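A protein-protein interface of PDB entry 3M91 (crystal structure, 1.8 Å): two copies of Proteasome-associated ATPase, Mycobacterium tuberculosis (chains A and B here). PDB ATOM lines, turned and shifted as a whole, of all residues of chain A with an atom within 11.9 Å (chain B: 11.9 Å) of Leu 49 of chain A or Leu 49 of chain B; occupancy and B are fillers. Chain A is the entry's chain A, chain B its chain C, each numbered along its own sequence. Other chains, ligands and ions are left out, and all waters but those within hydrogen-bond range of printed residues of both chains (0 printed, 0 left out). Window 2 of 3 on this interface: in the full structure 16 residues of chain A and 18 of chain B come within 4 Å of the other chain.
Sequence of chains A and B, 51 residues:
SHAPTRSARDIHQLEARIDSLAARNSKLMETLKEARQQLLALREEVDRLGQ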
ATOM      1  N   LEU A  39      -7.105  -5.962  10.825  1.00  0.00           N
ATOM      2  CA  LEU A  39      -7.865  -6.727   9.856  1.00  0.00           C
ATOM      3  C   LEU A  39      -8.502  -7.981  10.495  1.00  0.00           C
ATOM      4  O   LEU A  39      -9.624  -8.375  10.150  1.00  0.00           O
ATOM      5  CB  LEU A  39      -6.993  -7.214   8.691  1.00  0.00           C
ATOM      6  CG  LEU A  39      -6.576  -6.154   7.635  1.00  0.00           C
ATOM      7  CD1 LEU A  39      -5.258  -6.597   6.844  1.00  0.00           C
ATOM      8  CD2 LEU A  39      -7.738  -5.723   6.742  1.00  0.00           C
ATOM      9  N   LEU A  40      -7.712  -8.675  11.323  1.00  0.00           N
ATOM     10  CA  LEU A  40      -8.215  -9.857  11.969  1.00  0.00           C
ATOM     11  C   LEU A  40      -9.377  -9.460  12.884  1.00  0.00           C
ATOM     12  O   LEU A  40     -10.399 -10.173  12.949  1.00  0.00           O
ATOM     13  CB  LEU A  40      -7.063 -10.522  12.741  1.00  0.00           C
ATOM     14  CG  LEU A  40      -7.394 -11.794  13.522  1.00  0.00           C
ATOM     15  CD1 LEU A  40      -7.820 -12.913  12.486  1.00  0.00           C
ATOM     16  CD2 LEU A  40      -6.202 -12.301  14.450  1.00  0.00           C
ATOM     17  N   ALA A  41      -9.214  -8.401  13.668  1.00  0.00           N
ATOM     18  CA  ALA A  41     -10.313  -8.012  14.593  1.00  0.00           C
ATOM     19  C   ALA A  41     -11.599  -7.650  13.821  1.00  0.00           C
ATOM     20  O   ALA A  41     -12.688  -8.013  14.244  1.00  0.00           O
ATOM     21  CB  ALA A  41      -9.863  -6.825  15.519  1.00  0.00           C
ATOM     22  N   LEU A  42     -11.445  -7.030  12.648  1.00  0.00           N
ATOM     23  CA  LEU A  42     -12.640  -6.677  11.863  1.00  0.00           C
ATOM     24  C   LEU A  42     -13.237  -7.913  11.234  1.00  0.00           C
ATOM     25  O   LEU A  42     -14.431  -8.071  11.268  1.00  0.00           O
ATOM     26  CB  LEU A  42     -12.312  -5.683  10.759  1.00  0.00           C
ATOM     27  CG  LEU A  42     -12.068  -4.238  11.333  1.00  0.00           C
ATOM     28  CD1 LEU A  42     -11.325  -3.387  10.227  1.00  0.00           C
ATOM     29  CD2 LEU A  42     -13.370  -3.522  11.787  1.00  0.00           C
ATOM     30  N   ARG A  43     -12.374  -8.808  10.742  1.00  0.00           N
ATOM     31  CA  ARG A  43     -12.942 -10.092  10.189  1.00  0.00           C
ATOM     32  C   ARG A  43     -13.723 -10.838  11.288  1.00  0.00           C
ATOM     33  O   ARG A  43     -14.788 -11.361  11.023  1.00  0.00           O
ATOM     34  CB  ARG A  43     -11.795 -10.949   9.685  1.00  0.00           C
ATOM     35  CG  ARG A  43     -12.351 -12.177   8.836  1.00  0.00           C
ATOM     36  CD  ARG A  43     -11.238 -13.314   8.752  1.00  0.00           C
ATOM     37  NE  ARG A  43     -11.133 -14.019  10.021  1.00  0.00           N
ATOM     38  CZ  ARG A  43     -10.097 -14.745  10.416  1.00  0.00           C
ATOM     39  NH1 ARG A  43      -9.060 -14.954   9.635  1.00  0.00           N
ATOM     40  NH2 ARG A  43     -10.119 -15.286  11.652  1.00  0.00           N
ATOM     41  N   GLU A  44     -13.239 -10.934  12.525  1.00  0.00           N
ATOM     42  CA  GLU A  44     -13.980 -11.602  13.605  1.00  0.00           C
ATOM     43  C   GLU A  44     -15.340 -10.920  13.916  1.00  0.00           C
ATOM     44  O   GLU A  44     -16.354 -11.604  14.164  1.00  0.00           O
ATOM     45  CB  GLU A  44     -13.124 -11.568  14.896  1.00  0.00           C
ATOM     46  CG  GLU A  44     -11.809 -12.326  14.754  1.00  0.00           C
ATOM     47  CD  GLU A  44     -11.986 -13.831  14.881  1.00  0.00           C
ATOM     48  OE1 GLU A  44     -12.967 -14.311  15.518  1.00  0.00           O
ATOM     49  OE2 GLU A  44     -11.081 -14.557  14.390  1.00  0.00           O
ATOM     50  N   GLU A  45     -15.355  -9.569  13.789  1.00  0.00           N
ATOM     51  CA  GLU A  45     -16.599  -8.823  14.101  1.00  0.00           C
ATOM     52  C   GLU A  45     -17.564  -9.063  12.955  1.00  0.00           C
ATOM     53  O   GLU A  45     -18.789  -9.263  13.171  1.00  0.00           O
ATOM     54  CB  GLU A  45     -16.324  -7.375  14.201  1.00  0.00           C
ATOM     55  CG  GLU A  45     -17.635  -6.506  14.480  1.00  0.00           C
ATOM     56  CD  GLU A  45     -18.187  -6.738  15.881  1.00  0.00           C
ATOM     57  OE1 GLU A  45     -19.329  -6.385  16.123  1.00  0.00           O
ATOM     58  OE2 GLU A  45     -17.531  -7.334  16.717  1.00  0.00           O
ATOM     59  N   VAL A  46     -17.031  -9.097  11.726  1.00  0.00           N
ATOM     60  CA  VAL A  46     -17.921  -9.421  10.570  1.00  0.00           C
ATOM     61  C   VAL A  46     -18.605 -10.798  10.737  1.00  0.00           C
ATOM     62  O   VAL A  46     -19.862 -10.980  10.554  1.00  0.00           O
ATOM     63  CB  VAL A  46     -17.177  -9.270   9.241  1.00  0.00           C
ATOM     64  CG1 VAL A  46     -18.011  -9.903   8.074  1.00  0.00           C
ATOM     65  CG2 VAL A  46     -16.923  -7.722   8.873  1.00  0.00           C
ATOM     66  N   ASP A  47     -17.793 -11.802  11.181  1.00  0.00           N
ATOM     67  CA  ASP A  47     -18.339 -13.127  11.346  1.00  0.00           C
ATOM     68  C   ASP A  47     -19.300 -13.164  12.534  1.00  0.00           C
ATOM     69  O   ASP A  47     -20.239 -13.976  12.475  1.00  0.00           O
ATOM     70  CB  ASP A  47     -17.180 -14.138  11.547  1.00  0.00           C
ATOM     71  CG  ASP A  47     -16.515 -14.480  10.237  1.00  0.00           C
ATOM     72  OD1 ASP A  47     -17.128 -14.190   9.194  1.00  0.00           O
ATOM     73  OD2 ASP A  47     -15.374 -14.964  10.275  1.00  0.00           O
ATOM     74  N   ARG A  48     -19.081 -12.335  13.582  1.00  0.00           N
ATOM     75  CA  ARG A  48     -19.992 -12.312  14.710  1.00  0.00           C
ATOM     76  C   ARG A  48     -21.291 -11.620  14.258  1.00  0.00           C
ATOM     77  O   ARG A  48     -22.362 -11.979  14.708  1.00  0.00           O
ATOM     78  CB  ARG A  48     -19.433 -11.460  15.871  1.00  0.00           C
ATOM     79  CG  ARG A  48     -18.802 -12.284  16.882  1.00  0.00           C
ATOM     80  CD  ARG A  48     -18.545 -11.469  18.215  1.00  0.00           C
ATOM     81  NE  ARG A  48     -17.687 -10.364  17.875  1.00  0.00           N
ATOM     82  CZ  ARG A  48     -16.340 -10.397  17.805  1.00  0.00           C
ATOM     83  NH1 ARG A  48     -15.652 -11.489  18.125  1.00  0.00           N
ATOM     84  NH2 ARG A  48     -15.693  -9.305  17.444  1.00  0.00           N
ATOM     85  N   LEU A  49     -21.225 -10.647  13.378  1.00  0.00           N
ATOM     86  CA  LEU A  49     -22.431  -9.863  13.095  1.00  0.00           C
ATOM     87  C   LEU A  49     -23.289 -10.628  12.113  1.00  0.00           C
ATOM     88  O   LEU A  49     -24.510 -10.576  12.231  1.00  0.00           O
ATOM     89  CB  LEU A  49     -22.116  -8.410  12.665  1.00  0.00           C
ATOM     90  CG  LEU A  49     -21.503  -7.455  13.687  1.00  0.00           C
ATOM     91  CD1 LEU A  49     -20.991  -6.229  12.901  1.00  0.00           C
ATOM     92  CD2 LEU A  49     -22.410  -6.977  14.932  1.00  0.00           C
ATOM     93  N   GLY A  50     -22.666 -11.398  11.223  1.00  0.00           N
ATOM     94  CA  GLY A  50     -23.356 -12.218  10.238  1.00  0.00           C
ATOM     95  C   GLY A  50     -23.699 -13.607  10.787  1.00  0.00           C
ATOM     96  O   GLY A  50     -23.873 -14.574  10.034  1.00  0.00           O
ATOM     97  N   GLN A  51     -23.820 -13.755  12.105  1.00  0.00           N
ATOM     98  CA  GLN A  51     -24.003 -15.109  12.696  1.00  0.00           C
ATOM     99  C   GLN A  51     -25.393 -15.318  13.321  1.00  0.00           C
ATOM    100  O   GLN A  51     -26.014 -14.371  13.815  1.00  0.00           O
ATOM    101  CB  GLN A  51     -22.883 -15.404  13.711  1.00  0.00           C
ATOM    102  CG  GLN A  51     -23.175 -16.508  14.715  1.00  0.00           C
ATOM    103  CD  GLN A  51     -22.537 -16.225  16.083  1.00  0.00           C
ATOM    104  OE1 GLN A  51     -21.416 -15.670  16.170  1.00  0.00           O
ATOM    105  NE2 GLN A  51     -23.251 -16.613  17.166  1.00  0.00           N
ATOM    106  N   LEU B  39      -9.146  -2.690   5.016  1.00  0.00           N
ATOM    107  CA  LEU B  39      -9.651  -2.172   6.281  1.00  0.00           C
ATOM    108  C   LEU B  39     -10.903  -1.326   6.092  1.00  0.00           C
ATOM    109  O   LEU B  39     -11.853  -1.389   6.913  1.00  0.00           O
ATOM    110  CB  LEU B  39      -8.582  -1.271   6.986  1.00  0.00           C
ATOM    111  CG  LEU B  39      -7.398  -2.012   7.680  1.00  0.00           C
ATOM    112  CD1 LEU B  39      -6.250  -1.000   7.972  1.00  0.00           C
ATOM    113  CD2 LEU B  39      -7.874  -2.747   8.913  1.00  0.00           C
ATOM    114  N   LEU B  40     -10.880  -0.459   5.069  1.00  0.00           N
ATOM    115  CA  LEU B  40     -12.041   0.358   4.796  1.00  0.00           C
ATOM    116  C   LEU B  40     -13.258  -0.519   4.410  1.00  0.00           C
ATOM    117  O   LEU B  40     -14.414  -0.301   4.835  1.00  0.00           O
ATOM    118  CB  LEU B  40     -11.650   1.345   3.660  1.00  0.00           C
ATOM    119  CG  LEU B  40     -12.778   2.299   3.185  1.00  0.00           C
ATOM    120  CD1 LEU B  40     -13.138   3.269   4.363  1.00  0.00           C
ATOM    121  CD2 LEU B  40     -12.368   3.098   1.887  1.00  0.00           C
ATOM    122  N   ALA B  41     -13.031  -1.489   3.520  1.00  0.00           N
ATOM    123  CA  ALA B  41     -14.137  -2.378   3.085  1.00  0.00           C
ATOM    124  C   ALA B  41     -14.698  -3.136   4.299  1.00  0.00           C
ATOM    125  O   ALA B  41     -15.916  -3.279   4.422  1.00  0.00           O
ATOM    126  CB  ALA B  41     -13.646  -3.376   2.012  1.00  0.00           C
ATOM    127  N   LEU B  42     -13.851  -3.569   5.234  1.00  0.00           N
ATOM    128  CA  LEU B  42     -14.414  -4.273   6.395  1.00  0.00           C
ATOM    129  C   LEU B  42     -15.109  -3.297   7.349  1.00  0.00           C
ATOM    130  O   LEU B  42     -16.138  -3.621   7.906  1.00  0.00           O
ATOM    131  CB  LEU B  42     -13.295  -4.951   7.198  1.00  0.00           C
ATOM    132  CG  LEU B  42     -12.725  -6.182   6.420  1.00  0.00           C
ATOM    133  CD1 LEU B  42     -11.345  -6.560   7.142  1.00  0.00           C
ATOM    134  CD2 LEU B  42     -13.721  -7.318   6.499  1.00  0.00           C
ATOM    135  N   ARG B  43     -14.555  -2.097   7.520  1.00  0.00           N
ATOM    136  CA  ARG B  43     -15.297  -1.111   8.361  1.00  0.00           C
ATOM    137  C   ARG B  43     -16.685  -0.850   7.778  1.00  0.00           C
ATOM    138  O   ARG B  43     -17.647  -0.763   8.527  1.00  0.00           O
ATOM    139  CB  ARG B  43     -14.479   0.175   8.422  1.00  0.00           C
ATOM    140  CG  ARG B  43     -15.038   1.155   9.558  1.00  0.00           C
ATOM    141  CD  ARG B  43     -14.546   2.633   9.254  1.00  0.00           C
ATOM    142  NE  ARG B  43     -15.245   3.208   8.111  1.00  0.00           N
ATOM    143  CZ  ARG B  43     -14.838   4.210   7.386  1.00  0.00           C
ATOM    144  NH1 ARG B  43     -13.762   4.930   7.730  1.00  0.00           N
ATOM    145  NH2 ARG B  43     -15.623   4.603   6.367  1.00  0.00           N
ATOM    146  N   GLU B  44     -16.839  -0.676   6.448  1.00  0.00           N
ATOM    147  CA  GLU B  44     -18.160  -0.433   5.865  1.00  0.00           C
ATOM    148  C   GLU B  44     -19.088  -1.625   6.082  1.00  0.00           C
ATOM    149  O   GLU B  44     -20.288  -1.432   6.367  1.00  0.00           O
ATOM    150  CB  GLU B  44     -18.042  -0.224   4.308  1.00  0.00           C
ATOM    151  CG  GLU B  44     -17.166   0.971   4.000  1.00  0.00           C
ATOM    152  CD  GLU B  44     -17.946   2.273   4.055  1.00  0.00           C
ATOM    153  OE1 GLU B  44     -19.204   2.240   3.935  1.00  0.00           O
ATOM    154  OE2 GLU B  44     -17.317   3.349   4.206  1.00  0.00           O
ATOM    155  N   GLU B  45     -18.506  -2.825   6.073  1.00  0.00           N
ATOM    156  CA  GLU B  45     -19.399  -4.013   6.247  1.00  0.00           C
ATOM    157  C   GLU B  45     -19.835  -4.080   7.729  1.00  0.00           C
ATOM    158  O   GLU B  45     -21.015  -4.400   8.052  1.00  0.00           O
ATOM    159  CB  GLU B  45     -18.660  -5.244   5.824  1.00  0.00           C
ATOM    160  CG  GLU B  45     -19.509  -6.544   6.080  1.00  0.00           C
ATOM    161  CD  GLU B  45     -20.640  -6.739   5.103  1.00  0.00           C
ATOM    162  OE1 GLU B  45     -21.401  -7.668   5.305  1.00  0.00           O
ATOM    163  OE2 GLU B  45     -20.802  -5.990   4.168  1.00  0.00           O
ATOM    164  N   VAL B  46     -18.929  -3.756   8.637  1.00  0.00           N
ATOM    165  CA  VAL B  46     -19.289  -3.727  10.038  1.00  0.00           C
ATOM    166  C   VAL B  46     -20.410  -2.692  10.300  1.00  0.00           C
ATOM    167  O   VAL B  46     -21.350  -2.982  10.977  1.00  0.00           O
ATOM    168  CB  VAL B  46     -18.093  -3.458  10.943  1.00  0.00           C
ATOM    169  CG1 VAL B  46     -18.526  -3.112  12.301  1.00  0.00           C
ATOM    170  CG2 VAL B  46     -17.127  -4.637  10.971  1.00  0.00           C
ATOM    171  N   ASP B  47     -20.299  -1.516   9.711  1.00  0.00           N
ATOM    172  CA  ASP B  47     -21.376  -0.521   9.802  1.00  0.00           C
ATOM    173  C   ASP B  47     -22.661  -0.993   9.156  1.00  0.00           C
ATOM    174  O   ASP B  47     -23.748  -0.588   9.644  1.00  0.00           O
ATOM    175  CB  ASP B  47     -20.883   0.827   9.235  1.00  0.00           C
ATOM    176  CG  ASP B  47     -19.954   1.509  10.190  1.00  0.00           C
ATOM    177  OD1 ASP B  47     -19.954   1.131  11.379  1.00  0.00           O
ATOM    178  OD2 ASP B  47     -19.200   2.387   9.781  1.00  0.00           O
ATOM    179  N   ARG B  48     -22.600  -1.775   8.052  1.00  0.00           N
ATOM    180  CA  ARG B  48     -23.825  -2.232   7.411  1.00  0.00           C
ATOM    181  C   ARG B  48     -24.423  -3.308   8.328  1.00  0.00           C
ATOM    182  O   ARG B  48     -25.635  -3.420   8.474  1.00  0.00           O
ATOM    183  CB  ARG B  48     -23.514  -2.905   6.062  1.00  0.00           C
ATOM    184  CG  ARG B  48     -23.753  -1.951   4.960  1.00  0.00           C
ATOM    185  CD  ARG B  48     -23.787  -2.744   3.604  1.00  0.00           C
ATOM    186  NE  ARG B  48     -22.502  -3.388   3.478  1.00  0.00           N
ATOM    187  CZ  ARG B  48     -21.389  -2.821   2.964  1.00  0.00           C
ATOM    188  NH1 ARG B  48     -21.376  -1.579   2.460  1.00  0.00           N
ATOM    189  NH2 ARG B  48     -20.281  -3.526   2.932  1.00  0.00           N
ATOM    190  N   LEU B  49     -23.600  -4.097   8.963  1.00  0.00           N
ATOM    191  CA  LEU B  49     -24.113  -5.247   9.699  1.00  0.00           C
ATOM    192  C   LEU B  49     -24.725  -4.814  10.993  1.00  0.00           C
ATOM    193  O   LEU B  49     -25.706  -5.413  11.432  1.00  0.00           O
ATOM    194  CB  LEU B  49     -23.012  -6.296   9.955  1.00  0.00           C
ATOM    195  CG  LEU B  49     -22.621  -7.064   8.714  1.00  0.00           C
ATOM    196  CD1 LEU B  49     -21.326  -7.824   9.114  1.00  0.00           C
ATOM    197  CD2 LEU B  49     -23.706  -8.037   8.326  1.00  0.00           C
ATOM    198  N   GLY B  50     -24.162  -3.773  11.594  1.00  0.00           N
ATOM    199  CA  GLY B  50     -24.638  -3.235  12.848  1.00  0.00           C
ATOM    200  C   GLY B  50     -25.846  -2.313  12.699  1.00  0.00           C
ATOM    201  O   GLY B  50     -26.495  -2.012  13.701  1.00  0.00           O
ATOM    202  N   GLN B  51     -26.187  -1.859  11.482  1.00  0.00           N
ATOM    203  CA  GLN B  51     -27.272  -0.842  11.296  1.00  0.00           C
ATOM    204  C   GLN B  51     -28.677  -1.441  11.186  1.00  0.00           C
ATOM    205  O   GLN B  51     -28.996  -2.111  10.196  1.00  0.00           O
ATOM    206  CB  GLN B  51     -26.993   0.105  10.095  1.00  0.00           C
ATOM    207  CG  GLN B  51     -27.593  -0.312   8.711  1.00  0.00           C
ATOM    208  CD  GLN B  51     -26.849   0.302   7.492  1.00  0.00           C
ATOM    209  OE1 GLN B  51     -25.899   1.101   7.644  1.00  0.00           O
ATOM    210  NE2 GLN B  51     -27.291  -0.073   6.277  1.00  0.00           N
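Among the printed residues, merely in contact across the chains: Leu 39 of chain A with Leu 39 of chain B (3.7 Å), Leu 39 of chain A with Leu 42 of chain B (3.7 Å), Leu 42 of chain A with Leu 39 of chain B (3.7 Å), Leu 42 of chain A with Leu 42 of chain B (3.8 Å), Val 46 of chain A with Glu 45 of chain B (3.98 Å), Val 46 of chain A with Val 46 of chain B (3.7 Å), Val 46 of chain A with Leu 49 of chain B (3.8 Å), Leu 49 of chain A with Val 46 of chain B (3.8 Å) and Leu 49 of chain A with Leu 49 of chain B (3.6 Å).
Printed residues of chain B within 4 Å of Leu 39 of chain A: Leu 39 (3.7 Å) and Leu 42 (3.7 Å). Of the printed residues of chain B, Val 46 of chain A touches Glu 45 (3.98 Å), Val 46 (3.7 Å) and Leu 49 (3.8 Å). Leu 49 of chain A touches just these residues of chain B: Val 46 (3.8 Å) and Leu 49 (3.6 Å). No residue of chain B comes within 4 Å of Gln 51 of chain A. No residue of chain A comes within 4 Å of Arg 48 of chain B. Leu 49 of chain B touches just these residues of chain A: Val 46 and Leu 49. No residue of chain A comes within 4 Å of Gly 50 of chain B. The nearest residue of chain A that does not touch Leu 49 of chain B is Gly 50 of chain A (4.4 Å).
Printed residues of chain B that touch a printed residue of chain A: Leu 39, Leu 42, Glu 45, Val 46 and Leu 49. Hydrophobic or aromatic side chains of chain B that line the printed part of chain A: Leu 39, Leu 42, Val 46 and Leu 49. Of the 13 printed residues of chain A, 4 touch a printed residue of chain B. Among the printed residues, no Asp or Glu carboxylate lies within 4 Å of a Lys or Arg side-chain nitrogen of the other chain.
Leu 39 of chain A touches Leu 42 of chain B, and with the chains exchanged Leu 42 of chain A touches Leu 39 of chain B. Leu 42 of chain B touches its own counterpart, Leu 42 of chain A. Val 46 of chain A touches its own counterpart, Val 46 of chain B. Val 46 of chain A touches Leu 49 of chain B, and with the chains exchanged Leu 49 of chain A touches Val 46 of chain B. Of the 9 pairs that touch across the chains among the printed residues, 8 have their exchanged pair printed and touching as well.
NH2 of Arg 48 of chain B lies within salt-bridge range of OE2 of Glu 45 of chain B (2.8 Å).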
